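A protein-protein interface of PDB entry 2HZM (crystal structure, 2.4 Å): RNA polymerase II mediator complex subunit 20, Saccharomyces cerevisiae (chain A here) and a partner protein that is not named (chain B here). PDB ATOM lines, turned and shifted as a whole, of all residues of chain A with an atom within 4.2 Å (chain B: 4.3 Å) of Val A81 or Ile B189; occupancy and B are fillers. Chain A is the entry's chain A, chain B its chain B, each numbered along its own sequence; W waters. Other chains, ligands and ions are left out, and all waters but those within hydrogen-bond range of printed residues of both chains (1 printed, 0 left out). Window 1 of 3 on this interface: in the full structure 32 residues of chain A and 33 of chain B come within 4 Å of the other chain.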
ATOM      1  N   THR A  71      23.435   8.101   5.177  1.00  0.00           N
ATOM      2  CA  THR A  71      22.347   8.464   6.051  1.00  0.00           C
ATOM      3  C   THR A  71      22.786   9.498   7.040  1.00  0.00           C
ATOM      4  O   THR A  71      23.779   9.313   7.738  1.00  0.00           O
ATOM      5  CB  THR A  71      21.828   7.233   6.829  1.00  0.00           C
ATOM      6  OG1 THR A  71      21.545   6.172   5.907  1.00  0.00           O
ATOM      7  CG2 THR A  71      20.564   7.573   7.606  1.00  0.00           C
ATOM      8  N   MET A  80      24.718  14.109  12.067  1.00  0.00           N
ATOM      9  CA  MET A  80      25.796  13.140  12.080  1.00  0.00           C
ATOM     10  C   MET A  80      25.684  12.429  10.731  1.00  0.00           C
ATOM     11  O   MET A  80      24.615  11.931  10.363  1.00  0.00           O
ATOM     12  CB  MET A  80      25.578  12.168  13.249  1.00  0.00           C
ATOM     13  CG  MET A  80      26.658  11.106  13.460  1.00  0.00           C
ATOM     14  SD  MET A  80      26.298  10.058  14.951  1.00  0.00           S
ATOM     15  CE  MET A  80      25.333   8.799  14.205  1.00  0.00           C
ATOM     16  N   VAL A  81      26.769  12.411   9.973  1.00  0.00           N
ATOM     17  CA  VAL A  81      26.748  11.737   8.685  1.00  0.00           C
ATOM     18  C   VAL A  81      27.322  10.334   8.869  1.00  0.00           C
ATOM     19  O   VAL A  81      28.389  10.176   9.493  1.00  0.00           O
ATOM     20  CB  VAL A  81      27.583  12.521   7.633  1.00  0.00           C
ATOM     21  CG1 VAL A  81      27.351  11.962   6.259  1.00  0.00           C
ATOM     22  CG2 VAL A  81      27.205  13.990   7.652  1.00  0.00           C
ATOM     23  N   THR A  82      26.624   9.323   8.333  1.00  0.00           N
ATOM     24  CA  THR A  82      27.048   7.923   8.442  1.00  0.00           C
ATOM     25  C   THR A  82      26.898   7.213   7.123  1.00  0.00           C
ATOM     26  O   THR A  82      26.163   7.671   6.251  1.00  0.00           O
ATOM     27  CB  THR A  82      26.186   7.114   9.450  1.00  0.00           C
ATOM     28  OG1 THR A  82      24.846   6.979   8.940  1.00  0.00           O
ATOM     29  CG2 THR A  82      26.159   7.785  10.810  1.00  0.00           C
ATOM     30  N   ILE A 199      26.200  18.010   2.853  1.00  0.00           N
ATOM     31  CA  ILE A 199      25.214  16.957   3.025  1.00  0.00           C
ATOM     32  C   ILE A 199      24.387  17.144   4.294  1.00  0.00           C
ATOM     33  O   ILE A 199      23.199  16.827   4.324  1.00  0.00           O
ATOM     34  CB  ILE A 199      25.853  15.564   3.007  1.00  0.00           C
ATOM     35  CG1 ILE A 199      24.753  14.545   2.695  1.00  0.00           C
ATOM     36  CG2 ILE A 199      26.571  15.274   4.344  1.00  0.00           C
ATOM     37  CD1 ILE A 199      25.244  13.201   2.221  1.00  0.00           C
ATOM     38  N   CYS A 200      24.989  17.690   5.334  1.00  0.00           N
ATOM     39  CA  CYS A 200      24.238  17.918   6.560  1.00  0.00           C
ATOM     40  C   CYS A 200      23.218  19.043   6.378  1.00  0.00           C
ATOM     41  O   CYS A 200      22.096  18.939   6.874  1.00  0.00           O
ATOM     42  CB  CYS A 200      25.184  18.248   7.728  1.00  0.00           C
ATOM     43  SG  CYS A 200      26.101  16.797   8.382  1.00  0.00           S
ATOM     44  N   CYS B 160      33.040  16.249  13.794  1.00  0.00           N
ATOM     45  CA  CYS B 160      33.787  15.232  14.495  1.00  0.00           C
ATOM     46  C   CYS B 160      34.627  14.577  13.393  1.00  0.00           C
ATOM     47  O   CYS B 160      34.399  14.809  12.196  1.00  0.00           O
ATOM     48  CB  CYS B 160      32.849  14.197  15.110  1.00  0.00           C
ATOM     49  SG  CYS B 160      31.907  13.260  13.905  1.00  0.00           S
ATOM     50  N   SER B 161      35.606  13.780  13.793  1.00  0.00           N
ATOM     51  CA  SER B 161      36.439  13.075  12.832  1.00  0.00           C
ATOM     52  C   SER B 161      35.661  11.815  12.434  1.00  0.00           C
ATOM     53  O   SER B 161      34.545  11.586  12.887  1.00  0.00           O
ATOM     54  CB  SER B 161      37.733  12.632  13.502  1.00  0.00           C
ATOM     55  OG  SER B 161      37.426  11.634  14.471  1.00  0.00           O
ATOM     56  N   PRO B 162      36.227  11.013  11.539  1.00  0.00           N
ATOM     57  CA  PRO B 162      35.539   9.783  11.139  1.00  0.00           C
ATOM     58  C   PRO B 162      35.710   8.751  12.256  1.00  0.00           C
ATOM     59  O   PRO B 162      36.769   8.693  12.864  1.00  0.00           O
ATOM     60  CB  PRO B 162      36.292   9.359   9.880  1.00  0.00           C
ATOM     61  CG  PRO B 162      36.709  10.669   9.288  1.00  0.00           C
ATOM     62  CD  PRO B 162      37.144  11.483  10.481  1.00  0.00           C
ATOM     63  N   TRP B 163      34.686   7.951  12.544  1.00  0.00           N
ATOM     64  CA  TRP B 163      34.809   6.908  13.567  1.00  0.00           C
ATOM     65  C   TRP B 163      34.062   5.678  13.130  1.00  0.00           C
ATOM     66  O   TRP B 163      33.045   5.768  12.448  1.00  0.00           O
ATOM     67  CB  TRP B 163      34.178   7.280  14.924  1.00  0.00           C
ATOM     68  CG  TRP B 163      34.768   8.399  15.692  1.00  0.00           C
ATOM     69  CD1 TRP B 163      34.489   9.720  15.546  1.00  0.00           C
ATOM     70  CD2 TRP B 163      35.729   8.302  16.762  1.00  0.00           C
ATOM     71  NE1 TRP B 163      35.216  10.459  16.457  1.00  0.00           N
ATOM     72  CE2 TRP B 163      35.982   9.614  17.214  1.00  0.00           C
ATOM     73  CE3 TRP B 163      36.396   7.232  17.383  1.00  0.00           C
ATOM     74  CZ2 TRP B 163      36.878   9.893  18.256  1.00  0.00           C
ATOM     75  CZ3 TRP B 163      37.289   7.509  18.425  1.00  0.00           C
ATOM     76  CH2 TRP B 163      37.520   8.829  18.850  1.00  0.00           C
ATOM     77  N   LEU B 165      31.704   2.794  14.323  1.00  0.00           N
ATOM     78  CA  LEU B 165      30.800   2.616  15.433  1.00  0.00           C
ATOM     79  C   LEU B 165      30.388   1.153  15.451  1.00  0.00           C
ATOM     80  O   LEU B 165      29.855   0.636  14.469  1.00  0.00           O
ATOM     81  CB  LEU B 165      29.587   3.554  15.264  1.00  0.00           C
ATOM     82  CG  LEU B 165      28.544   3.493  16.384  1.00  0.00           C
ATOM     83  CD1 LEU B 165      27.597   4.691  16.335  1.00  0.00           C
ATOM     84  CD2 LEU B 165      27.785   2.201  16.245  1.00  0.00           C
ATOM     85  N   THR B 187      28.712   0.491  11.679  1.00  0.00           N
ATOM     86  CA  THR B 187      28.401   1.535  10.728  1.00  0.00           C
ATOM     87  C   THR B 187      29.538   2.531  10.889  1.00  0.00           C
ATOM     88  O   THR B 187      30.220   2.515  11.896  1.00  0.00           O
ATOM     89  CB  THR B 187      27.008   2.205  10.962  1.00  0.00           C
ATOM     90  OG1 THR B 187      26.656   2.923   9.769  1.00  0.00           O
ATOM     91  CG2 THR B 187      27.033   3.173  12.161  1.00  0.00           C
ATOM     92  N   ILE B 188      29.750   3.369   9.883  1.00  0.00           N
ATOM     93  CA  ILE B 188      30.806   4.369   9.880  1.00  0.00           C
ATOM     94  C   ILE B 188      30.265   5.793  10.044  1.00  0.00           C
ATOM     95  O   ILE B 188      29.311   6.179   9.377  1.00  0.00           O
ATOM     96  CB  ILE B 188      31.583   4.287   8.535  1.00  0.00           C
ATOM     97  CG1 ILE B 188      32.197   2.882   8.384  1.00  0.00           C
ATOM     98  CG2 ILE B 188      32.664   5.386   8.452  1.00  0.00           C
ATOM     99  CD1 ILE B 188      33.302   2.574   9.426  1.00  0.00           C
ATOM    100  N   ILE B 189      30.851   6.565  10.956  1.00  0.00           N
ATOM    101  CA  ILE B 189      30.459   7.946  11.151  1.00  0.00           C
ATOM    102  C   ILE B 189      31.497   8.757  10.358  1.00  0.00           C
ATOM    103  O   ILE B 189      32.704   8.604  10.581  1.00  0.00           O
ATOM    104  CB  ILE B 189      30.541   8.360  12.632  1.00  0.00           C
ATOM    105  CG1 ILE B 189      29.467   7.632  13.450  1.00  0.00           C
ATOM    106  CG2 ILE B 189      30.339   9.877  12.770  1.00  0.00           C
ATOM    107  CD1 ILE B 189      29.619   7.895  14.956  1.00  0.00           C
ATOM    108  N   LEU B 190      31.044   9.618   9.443  1.00  0.00           N
ATOM    109  CA  LEU B 190      31.977  10.390   8.625  1.00  0.00           C
ATOM    110  C   LEU B 190      32.215  11.824   9.073  1.00  0.00           C
ATOM    111  O   LEU B 190      33.317  12.343   8.921  1.00  0.00           O
ATOM    112  CB  LEU B 190      31.511  10.412   7.168  1.00  0.00           C
ATOM    113  CG  LEU B 190      31.542   9.084   6.401  1.00  0.00           C
ATOM    114  CD1 LEU B 190      30.835   9.287   5.047  1.00  0.00           C
ATOM    115  CD2 LEU B 190      33.014   8.612   6.207  1.00  0.00           C
ATOM    116  N   SER B 191      31.187  12.469   9.610  1.00  0.00           N
ATOM    117  CA  SER B 191      31.310  13.847  10.048  1.00  0.00           C
ATOM    118  C   SER B 191      30.044  14.248  10.777  1.00  0.00           C
ATOM    119  O   SER B 191      29.104  13.466  10.893  1.00  0.00           O
ATOM    120  CB  SER B 191      31.532  14.777   8.836  1.00  0.00           C
ATOM    121  OG  SER B 191      30.404  14.778   7.956  1.00  0.00           O
ATOM    122  N   MET B 203      26.635  11.209  20.932  1.00  0.00           N
ATOM    123  CA  MET B 203      26.327  10.003  21.703  1.00  0.00           C
ATOM    124  C   MET B 203      25.298  10.309  22.805  1.00  0.00           C
ATOM    125  O   MET B 203      24.380   9.518  23.042  1.00  0.00           O
ATOM    126  CB  MET B 203      27.617   9.398  22.306  1.00  0.00           C
ATOM    127  CG  MET B 203      28.582   8.751  21.253  1.00  0.00           C
ATOM    128  SD  MET B 203      27.869   7.397  20.246  1.00  0.00           S
ATOM    129  CE  MET B 203      27.641   8.268  18.676  1.00  0.00           C
HETATM  130  O   HOH W   1      24.504   4.536   7.966  1.00  0.00           O
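N of Leu B190 sits at hydrogen-bond distance from O of Val A81, at 2.7 Å. The backbone carbonyl oxygen (O) of Ser B191 is in hydrogen-bond range of the backbone NH (N) of Val A81 (2.7 Å).
Water W1 lies within hydrogen-bond range of the side-chain hydroxyl (OG1) of Thr A82 (2.7 Å) and the side-chain hydroxyl (OG1) of Thr B187 (3.2 Å).
CG of Met A80 touches CG2 of Ile B189 (3.9 Å). Met A80 touches Ser B191 (CA to O, 3.5 Å). Val A81 touches Ile B189. Thr A82 touches Ile B188.
The side-chain hydroxyl (OG1) of Thr A82 is in hydrogen-bond range of the backbone carbonyl oxygen (O) of Thr A71, 2.8 Å away. O of Trp B163 lies within hydrogen-bond range of N of Ile B189 (2.8 Å).
Of the 11 printed residues of chain B, 4 touch a printed residue of chain A. Along chain B the printed residues that touch a printed residue of chain A span positions 188 to 191. Of the 6 printed residues of chain A, 3 touch a printed residue of chain B.
Of chain B, only Ile B189 (3.5 Å), Leu B190 (2.7 Å) and Ser B191 (2.7 Å) come within 4 Å of Val A81. Of chain A, only Met A80 and Val A81 come within 4 Å of Ile B189. Of the printed residues of chain A, Ser B191 touches Met A80 and Val A81. Printed residues of chain A within 4 Å of Ile B188: Thr A82. Of the printed residues of chain B, Thr A82 touches Ile B188 (3.0 Å). Printed residues of chain A within 4 Å of Leu B190: Val A81. Thr A71 touches none of the printed residues of chain B. The nearest printed residue of chain A that does not touch Ile B189 is Thr A82 (4.2 Å).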
